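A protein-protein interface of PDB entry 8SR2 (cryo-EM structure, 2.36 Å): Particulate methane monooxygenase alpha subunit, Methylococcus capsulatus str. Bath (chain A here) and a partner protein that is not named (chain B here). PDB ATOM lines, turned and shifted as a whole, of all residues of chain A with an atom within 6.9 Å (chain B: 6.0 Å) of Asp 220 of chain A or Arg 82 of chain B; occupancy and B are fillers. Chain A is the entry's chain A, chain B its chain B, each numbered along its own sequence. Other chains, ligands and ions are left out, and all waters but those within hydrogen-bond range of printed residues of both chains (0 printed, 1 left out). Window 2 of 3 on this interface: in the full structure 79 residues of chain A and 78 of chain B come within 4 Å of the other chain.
Asp 220 of chain A touches just one residue of chain B: Arg 82.
Of chain A, only Leu 216 (3.4 Å), Val 219 (3.7 Å) and Asp 220 (3.4 Å) come within 4 Å of Arg 82 of chain B.
Printed residues of chain B within 4 Å of Leu 227 of chain A: Arg 84 (3.8 Å).
Printed residues of chain A within 4 Å of Glu 81 of chain B: Val 219.
Arg 223 of chain A touches none of the printed residues of chain B.
The nearest printed residue of chain B that does not touch Phe 212 of chain A is Leu 79 of chain B (4.5 Å).
NE of Arg 215 of chain A lies within hydrogen-bond range of O of Tyr 83 of chain B, 2.7 Å away.
The side-chain carboxylate (OD1) of Asp 220 of chain A is in salt-bridge range of the guanidinium group (NH2) of Arg 82 of chain B.
NH2 of Arg 215 of chain A sits close to O of Arg 84 of chain B (2.4 Å).
Phe 212 of chain A touches Tyr 83 of chain B.
Leu 216 of chain A touches Arg 82 of chain B.
CE2 of Tyr 83 of chain B touches CB of Leu 216 of chain A, at 3.5 Å.
Val 219 of chain A touches Glu 81 of chain B.
Val 219 of chain A touches Arg 82 of chain B (CB to O, 3.7 Å).
Arg 84 of chain B touches Val 219 of chain A.
Arg 84 of chain B touches Leu 227 of chain A.
Of the 13 printed residues of chain A, 6 touch a printed residue of chain B.
Hydrophobic or aromatic side chains of chain A within 4 Å of the printed part of chain B: Leu 216, Val 219 and Leu 227.
Of the 11 printed residues of chain B, 4 touch a printed residue of chain A.
Printed residues of chain B that touch a printed residue of chain A: Glu 81, Arg 82, Tyr 83 and Arg 84.
Hydrophobic or aromatic side chains of chain B within 4 Å of the printed part of chain A: Tyr 83.
Among the printed residues, Asp or Glu carboxylates within 4 Å of a Lys or Arg side-chain nitrogen of the other chain: Asp 220 of chain A with Arg 82 of chain B (3.4 Å).
The backbone NH (N) of Arg 84 of chain B sits at hydrogen-bond distance from the backbone carbonyl oxygen (O) of Leu 79 of chain B, at 3.4 Å.
OH of Tyr 141 of chain B sits at hydrogen-bond distance from N of Glu 81 of chain B (3.2 Å).
NH1 of Arg 82 of chain B lies within salt-bridge range of OE2 of Glu 241 of chain B, at 2.7 Å.
The backbone carbonyl oxygen (O) of Leu 227 of chain A lies close to the guanidinium group (NH1) of Arg 215 of chain A, 3.4 Å away.
The backbone carbonyl oxygen of Trp 80 of chain B is in hydrogen-bond range of the guanidinium group of Arg 84 of chain B (2.4 Å).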
ATOM      1  N   PHE A 212      20.175  -8.073  21.516  1.00  0.00           N
ATOM      2  CA  PHE A 212      20.154  -9.037  20.416  1.00  0.00           C
ATOM      3  C   PHE A 212      21.060 -10.245  20.636  1.00  0.00           C
ATOM      4  O   PHE A 212      20.573 -11.376  20.713  1.00  0.00           O
ATOM      5  CB  PHE A 212      20.530  -8.327  19.109  1.00  0.00           C
ATOM      6  CG  PHE A 212      19.473  -7.386  18.608  1.00  0.00           C
ATOM      7  CD1 PHE A 212      18.276  -7.869  18.110  1.00  0.00           C
ATOM      8  CD2 PHE A 212      19.678  -6.016  18.641  1.00  0.00           C
ATOM      9  CE1 PHE A 212      17.301  -7.005  17.651  1.00  0.00           C
ATOM     10  CE2 PHE A 212      18.706  -5.148  18.182  1.00  0.00           C
ATOM     11  CZ  PHE A 212      17.517  -5.643  17.687  1.00  0.00           C
ATOM     12  N   PRO A 214      23.505 -11.444  23.123  1.00  0.00           N
ATOM     13  CA  PRO A 214      23.465 -12.313  24.313  1.00  0.00           C
ATOM     14  C   PRO A 214      22.130 -13.008  24.504  1.00  0.00           C
ATOM     15  O   PRO A 214      22.099 -14.177  24.906  1.00  0.00           O
ATOM     16  CB  PRO A 214      23.780 -11.348  25.464  1.00  0.00           C
ATOM     17  CG  PRO A 214      23.413 -10.017  24.949  1.00  0.00           C
ATOM     18  CD  PRO A 214      23.752 -10.040  23.499  1.00  0.00           C
ATOM     19  N   ARG A 215      21.018 -12.328  24.213  1.00  0.00           N
ATOM     20  CA  ARG A 215      19.712 -12.964  24.343  1.00  0.00           C
ATOM     21  C   ARG A 215      19.540 -14.082  23.321  1.00  0.00           C
ATOM     22  O   ARG A 215      18.999 -15.145  23.641  1.00  0.00           O
ATOM     23  CB  ARG A 215      18.600 -11.925  24.207  1.00  0.00           C
ATOM     24  CG  ARG A 215      18.429 -11.048  25.439  1.00  0.00           C
ATOM     25  CD  ARG A 215      17.303 -10.040  25.262  1.00  0.00           C
ATOM     26  NE  ARG A 215      15.991 -10.618  25.520  1.00  0.00           N
ATOM     27  CZ  ARG A 215      15.374 -10.576  26.692  1.00  0.00           C
ATOM     28  NH1 ARG A 215      15.928 -10.001  27.746  1.00  0.00           N
ATOM     29  NH2 ARG A 215      14.167 -11.124  26.808  1.00  0.00           N
ATOM     30  N   LEU A 216      20.002 -13.862  22.086  1.00  0.00           N
ATOM     31  CA  LEU A 216      19.951 -14.912  21.077  1.00  0.00           C
ATOM     32  C   LEU A 216      20.775 -16.119  21.500  1.00  0.00           C
ATOM     33  O   LEU A 216      20.342 -17.266  21.339  1.00  0.00           O
ATOM     34  CB  LEU A 216      20.449 -14.374  19.736  1.00  0.00           C
ATOM     35  CG  LEU A 216      20.632 -15.390  18.606  1.00  0.00           C
ATOM     36  CD1 LEU A 216      19.297 -15.989  18.197  1.00  0.00           C
ATOM     37  CD2 LEU A 216      21.324 -14.747  17.415  1.00  0.00           C
ATOM     38  N   LEU A 217      21.970 -15.880  22.043  1.00  0.00           N
ATOM     39  CA  LEU A 217      22.820 -16.988  22.468  1.00  0.00           C
ATOM     40  C   LEU A 217      22.213 -17.733  23.652  1.00  0.00           C
ATOM     41  O   LEU A 217      22.302 -18.962  23.725  1.00  0.00           O
ATOM     42  CB  LEU A 217      24.219 -16.476  22.799  1.00  0.00           C
ATOM     43  CG  LEU A 217      25.021 -16.049  21.570  1.00  0.00           C
ATOM     44  CD1 LEU A 217      26.233 -15.230  21.964  1.00  0.00           C
ATOM     45  CD2 LEU A 217      25.433 -17.262  20.752  1.00  0.00           C
ATOM     46  N   MET A 218      21.599 -16.985  24.561  1.00  0.00           N
ATOM     47  CA  MET A 218      20.964 -17.563  25.737  1.00  0.00           C
ATOM     48  C   MET A 218      19.785 -18.431  25.322  1.00  0.00           C
ATOM     49  O   MET A 218      19.587 -19.521  25.854  1.00  0.00           O
ATOM     50  CB  MET A 218      20.491 -16.462  26.684  1.00  0.00           C
ATOM     51  CG  MET A 218      21.616 -15.688  27.348  1.00  0.00           C
ATOM     52  SD  MET A 218      22.114 -16.417  28.919  1.00  0.00           S
ATOM     53  CE  MET A 218      20.522 -16.641  29.708  1.00  0.00           C
ATOM     54  N   VAL A 219      19.002 -17.936  24.369  1.00  0.00           N
ATOM     55  CA  VAL A 219      17.846 -18.669  23.874  1.00  0.00           C
ATOM     56  C   VAL A 219      18.292 -19.895  23.091  1.00  0.00           C
ATOM     57  O   VAL A 219      17.644 -20.937  23.124  1.00  0.00           O
ATOM     58  CB  VAL A 219      16.960 -17.790  22.973  1.00  0.00           C
ATOM     59  CG1 VAL A 219      15.902 -18.634  22.284  1.00  0.00           C
ATOM     60  CG2 VAL A 219      16.315 -16.679  23.786  1.00  0.00           C
ATOM     61  N   ASP A 220      19.408 -19.760  22.382  1.00  0.00           N
ATOM     62  CA  ASP A 220      19.957 -20.855  21.597  1.00  0.00           C
ATOM     63  C   ASP A 220      20.642 -21.860  22.512  1.00  0.00           C
ATOM     64  O   ASP A 220      20.141 -22.961  22.731  1.00  0.00           O
ATOM     65  CB  ASP A 220      20.955 -20.327  20.568  1.00  0.00           C
ATOM     66  CG  ASP A 220      20.281 -19.633  19.404  1.00  0.00           C
ATOM     67  OD1 ASP A 220      19.035 -19.557  19.396  1.00  0.00           O
ATOM     68  OD2 ASP A 220      20.997 -19.162  18.498  1.00  0.00           O
ATOM     69  N   ALA A 221      21.794 -21.470  23.045  1.00  0.00           N
ATOM     70  CA  ALA A 221      22.552 -22.334  23.940  1.00  0.00           C
ATOM     71  C   ALA A 221      21.758 -22.617  25.206  1.00  0.00           C
ATOM     72  O   ALA A 221      21.795 -21.844  26.162  1.00  0.00           O
ATOM     73  CB  ALA A 221      23.894 -21.705  24.281  1.00  0.00           C
ATOM     74  N   GLY A 222      21.037 -23.733  25.204  1.00  0.00           N
ATOM     75  CA  GLY A 222      20.235 -24.121  26.348  1.00  0.00           C
ATOM     76  C   GLY A 222      18.887 -23.430  26.357  1.00  0.00           C
ATOM     77  O   GLY A 222      18.547 -22.698  25.431  1.00  0.00           O
ATOM     78  N   ARG A 223      18.118 -23.664  27.413  1.00  0.00           N
ATOM     79  CA  ARG A 223      16.801 -23.058  27.544  1.00  0.00           C
ATOM     80  C   ARG A 223      16.919 -21.582  27.896  1.00  0.00           C
ATOM     81  O   ARG A 223      17.945 -21.136  28.409  1.00  0.00           O
ATOM     82  CB  ARG A 223      15.981 -23.787  28.608  1.00  0.00           C
ATOM     83  CG  ARG A 223      15.221 -24.998  28.092  1.00  0.00           C
ATOM     84  CD  ARG A 223      14.476 -25.704  29.214  1.00  0.00           C
ATOM     85  NE  ARG A 223      13.606 -26.763  28.714  1.00  0.00           N
ATOM     86  CZ  ARG A 223      13.406 -27.922  29.335  1.00  0.00           C
ATOM     87  NH1 ARG A 223      14.014 -28.173  30.485  1.00  0.00           N
ATOM     88  NH2 ARG A 223      12.597 -28.829  28.805  1.00  0.00           N
ATOM     89  N   ALA A 224      15.862 -20.828  27.611  1.00  0.00           N
ATOM     90  CA  ALA A 224      15.833 -19.404  27.907  1.00  0.00           C
ATOM     91  C   ALA A 224      15.462 -19.202  29.368  1.00  0.00           C
ATOM     92  O   ALA A 224      16.303 -19.361  30.251  1.00  0.00           O
ATOM     93  CB  ALA A 224      14.842 -18.691  27.003  1.00  0.00           C
ATOM     94  N   LEU A 227      15.699 -14.400  30.699  1.00  0.00           N
ATOM     95  CA  LEU A 227      15.638 -13.060  30.135  1.00  0.00           C
ATOM     96  C   LEU A 227      14.274 -12.439  30.410  1.00  0.00           C
ATOM     97  O   LEU A 227      14.096 -11.227  30.292  1.00  0.00           O
ATOM     98  CB  LEU A 227      15.906 -13.101  28.633  1.00  0.00           C
ATOM     99  CG  LEU A 227      16.868 -14.191  28.159  1.00  0.00           C
ATOM    100  CD1 LEU A 227      16.302 -14.919  26.950  1.00  0.00           C
ATOM    101  CD2 LEU A 227      18.232 -13.599  27.845  1.00  0.00           C
ATOM    102  N   SER B  77       6.642 -13.219  15.853  1.00  0.00           N
ATOM    103  CA  SER B  77       7.020 -14.616  15.681  1.00  0.00           C
ATOM    104  C   SER B  77       8.523 -14.794  15.546  1.00  0.00           C
ATOM    105  O   SER B  77       9.049 -15.847  15.921  1.00  0.00           O
ATOM    106  CB  SER B  77       6.320 -15.202  14.454  1.00  0.00           C
ATOM    107  OG  SER B  77       7.098 -15.013  13.287  1.00  0.00           O
ATOM    108  N   TYR B  78       9.224 -13.795  15.016  1.00  0.00           N
ATOM    109  CA  TYR B  78      10.682 -13.849  14.958  1.00  0.00           C
ATOM    110  C   TYR B  78      11.341 -13.391  16.253  1.00  0.00           C
ATOM    111  O   TYR B  78      12.147 -14.130  16.834  1.00  0.00           O
ATOM    112  CB  TYR B  78      11.192 -13.003  13.789  1.00  0.00           C
ATOM    113  CG  TYR B  78      12.670 -12.682  13.858  1.00  0.00           C
ATOM    114  CD1 TYR B  78      13.621 -13.634  13.517  1.00  0.00           C
ATOM    115  CD2 TYR B  78      13.112 -11.428  14.260  1.00  0.00           C
ATOM    116  CE1 TYR B  78      14.972 -13.348  13.576  1.00  0.00           C
ATOM    117  CE2 TYR B  78      14.460 -11.132  14.324  1.00  0.00           C
ATOM    118  CZ  TYR B  78      15.385 -12.098  13.979  1.00  0.00           C
ATOM    119  OH  TYR B  78      16.729 -11.809  14.040  1.00  0.00           O
ATOM    120  N   LEU B  79      11.016 -12.180  16.715  1.00  0.00           N
ATOM    121  CA  LEU B  79      11.722 -11.587  17.845  1.00  0.00           C
ATOM    122  C   LEU B  79      11.511 -12.390  19.122  1.00  0.00           C
ATOM    123  O   LEU B  79      12.472 -12.693  19.835  1.00  0.00           O
ATOM    124  CB  LEU B  79      11.275 -10.139  18.045  1.00  0.00           C
ATOM    125  CG  LEU B  79      11.854  -9.098  17.087  1.00  0.00           C
ATOM    126  CD1 LEU B  79      11.349  -7.710  17.439  1.00  0.00           C
ATOM    127  CD2 LEU B  79      13.373  -9.139  17.107  1.00  0.00           C
ATOM    128  N   TRP B  80      10.260 -12.732  19.440  1.00  0.00           N
ATOM    129  CA  TRP B  80      10.010 -13.488  20.659  1.00  0.00           C
ATOM    130  C   TRP B  80      10.709 -14.838  20.615  1.00  0.00           C
ATOM    131  O   TRP B  80      11.418 -15.215  21.554  1.00  0.00           O
ATOM    132  CB  TRP B  80       8.506 -13.665  20.871  1.00  0.00           C
ATOM    133  CG  TRP B  80       8.170 -14.464  22.091  1.00  0.00           C
ATOM    134  CD1 TRP B  80       7.648 -15.721  22.127  1.00  0.00           C
ATOM    135  CD2 TRP B  80       8.345 -14.062  23.455  1.00  0.00           C
ATOM    136  NE1 TRP B  80       7.479 -16.126  23.429  1.00  0.00           N
ATOM    137  CE2 TRP B  80       7.901 -15.126  24.263  1.00  0.00           C
ATOM    138  CE3 TRP B  80       8.832 -12.903  24.071  1.00  0.00           C
ATOM    139  CZ2 TRP B  80       7.928 -15.068  25.654  1.00  0.00           C
ATOM    140  CZ3 TRP B  80       8.858 -12.849  25.452  1.00  0.00           C
ATOM    141  CH2 TRP B  80       8.410 -13.924  26.227  1.00  0.00           C
ATOM    142  N   GLU B  81      10.573 -15.554  19.496  1.00  0.00           N
ATOM    143  CA  GLU B  81      11.140 -16.893  19.398  1.00  0.00           C
ATOM    144  C   GLU B  81      12.660 -16.879  19.476  1.00  0.00           C
ATOM    145  O   GLU B  81      13.258 -17.811  20.027  1.00  0.00           O
ATOM    146  CB  GLU B  81      10.684 -17.563  18.102  1.00  0.00           C
ATOM    147  CG  GLU B  81      10.678 -19.088  18.140  1.00  0.00           C
ATOM    148  CD  GLU B  81       9.535 -19.668  18.961  1.00  0.00           C
ATOM    149  OE1 GLU B  81       9.426 -19.358  20.166  1.00  0.00           O
ATOM    150  OE2 GLU B  81       8.739 -20.444  18.393  1.00  0.00           O
ATOM    151  N   ARG B  82      13.309 -15.843  18.937  1.00  0.00           N
ATOM    152  CA  ARG B  82      14.762 -15.858  18.855  1.00  0.00           C
ATOM    153  C   ARG B  82      15.467 -15.097  19.973  1.00  0.00           C
ATOM    154  O   ARG B  82      16.643 -15.372  20.227  1.00  0.00           O
ATOM    155  CB  ARG B  82      15.224 -15.302  17.502  1.00  0.00           C
ATOM    156  CG  ARG B  82      14.767 -16.122  16.305  1.00  0.00           C
ATOM    157  CD  ARG B  82      14.937 -17.614  16.546  1.00  0.00           C
ATOM    158  NE  ARG B  82      16.330 -17.987  16.774  1.00  0.00           N
ATOM    159  CZ  ARG B  82      17.202 -18.255  15.812  1.00  0.00           C
ATOM    160  NH1 ARG B  82      16.861 -18.200  14.536  1.00  0.00           N
ATOM    161  NH2 ARG B  82      18.446 -18.588  16.140  1.00  0.00           N
ATOM    162  N   TYR B  83      14.797 -14.156  20.644  1.00  0.00           N
ATOM    163  CA  TYR B  83      15.456 -13.357  21.666  1.00  0.00           C
ATOM    164  C   TYR B  83      14.625 -13.138  22.923  1.00  0.00           C
ATOM    165  O   TYR B  83      15.126 -12.503  23.858  1.00  0.00           O
ATOM    166  CB  TYR B  83      15.847 -11.977  21.102  1.00  0.00           C
ATOM    167  CG  TYR B  83      16.430 -11.986  19.709  1.00  0.00           C
ATOM    168  CD1 TYR B  83      15.611 -11.912  18.591  1.00  0.00           C
ATOM    169  CD2 TYR B  83      17.800 -12.046  19.510  1.00  0.00           C
ATOM    170  CE1 TYR B  83      16.139 -11.912  17.315  1.00  0.00           C
ATOM    171  CE2 TYR B  83      18.339 -12.046  18.238  1.00  0.00           C
ATOM    172  CZ  TYR B  83      17.504 -11.980  17.145  1.00  0.00           C
ATOM    173  OH  TYR B  83      18.040 -11.982  15.878  1.00  0.00           O
ATOM    174  N   ARG B  84      13.387 -13.632  22.981  1.00  0.00           N
ATOM    175  CA  ARG B  84      12.459 -13.321  24.070  1.00  0.00           C
ATOM    176  C   ARG B  84      12.289 -11.812  24.231  1.00  0.00           C
ATOM    177  O   ARG B  84      12.289 -11.275  25.342  1.00  0.00           O
ATOM    178  CB  ARG B  84      12.907 -13.971  25.382  1.00  0.00           C
ATOM    179  CG  ARG B  84      12.865 -15.488  25.356  1.00  0.00           C
ATOM    180  CD  ARG B  84      11.469 -16.002  25.675  1.00  0.00           C
ATOM    181  NE  ARG B  84      11.307 -17.417  25.357  1.00  0.00           N
ATOM    182  CZ  ARG B  84      11.266 -17.916  24.128  1.00  0.00           C
ATOM    183  NH1 ARG B  84      11.353 -17.137  23.061  1.00  0.00           N
ATOM    184  NH2 ARG B  84      11.131 -19.228  23.965  1.00  0.00           N
ATOM    185  N   TYR B 141       1.702 -18.979  21.071  1.00  0.00           N
ATOM    186  CA  TYR B 141       1.394 -18.156  19.911  1.00  0.00           C
ATOM    187  C   TYR B 141      -0.071 -18.307  19.542  1.00  0.00           C
ATOM    188  O   TYR B 141      -0.673 -17.408  18.962  1.00  0.00           O
ATOM    189  CB  TYR B 141       2.281 -18.537  18.726  1.00  0.00           C
ATOM    190  CG  TYR B 141       3.664 -17.933  18.790  1.00  0.00           C
ATOM    191  CD1 TYR B 141       3.863 -16.582  18.542  1.00  0.00           C
ATOM    192  CD2 TYR B 141       4.768 -18.712  19.102  1.00  0.00           C
ATOM    193  CE1 TYR B 141       5.123 -16.025  18.601  1.00  0.00           C
ATOM    194  CE2 TYR B 141       6.034 -18.162  19.164  1.00  0.00           C
ATOM    195  CZ  TYR B 141       6.204 -16.820  18.911  1.00  0.00           C
ATOM    196  OH  TYR B 141       7.462 -16.269  18.970  1.00  0.00           O
ATOM    197  N   SER B 239      12.153 -15.763   8.595  1.00  0.00           N
ATOM    198  CA  SER B 239      13.214 -15.903   9.581  1.00  0.00           C
ATOM    199  C   SER B 239      14.105 -17.110   9.323  1.00  0.00           C
ATOM    200  O   SER B 239      15.067 -17.318  10.069  1.00  0.00           O
ATOM    201  CB  SER B 239      12.617 -16.001  10.988  1.00  0.00           C
ATOM    202  OG  SER B 239      11.687 -14.958  11.219  1.00  0.00           O
ATOM    203  N   GLU B 241      17.083 -19.357   7.737  1.00  0.00           N
ATOM    204  CA  GLU B 241      18.489 -18.989   7.599  1.00  0.00           C
ATOM    205  C   GLU B 241      19.226 -19.911   6.633  1.00  0.00           C
ATOM    206  O   GLU B 241      20.379 -20.275   6.879  1.00  0.00           O
ATOM    207  CB  GLU B 241      19.182 -18.993   8.960  1.00  0.00           C
ATOM    208  CG  GLU B 241      18.709 -17.907   9.908  1.00  0.00           C
ATOM    209  CD  GLU B 241      18.573 -18.400  11.334  1.00  0.00           C
ATOM    210  OE1 GLU B 241      19.579 -18.876  11.900  1.00  0.00           O
ATOM    211  OE2 GLU B 241      17.457 -18.316  11.889  1.00  0.00           O
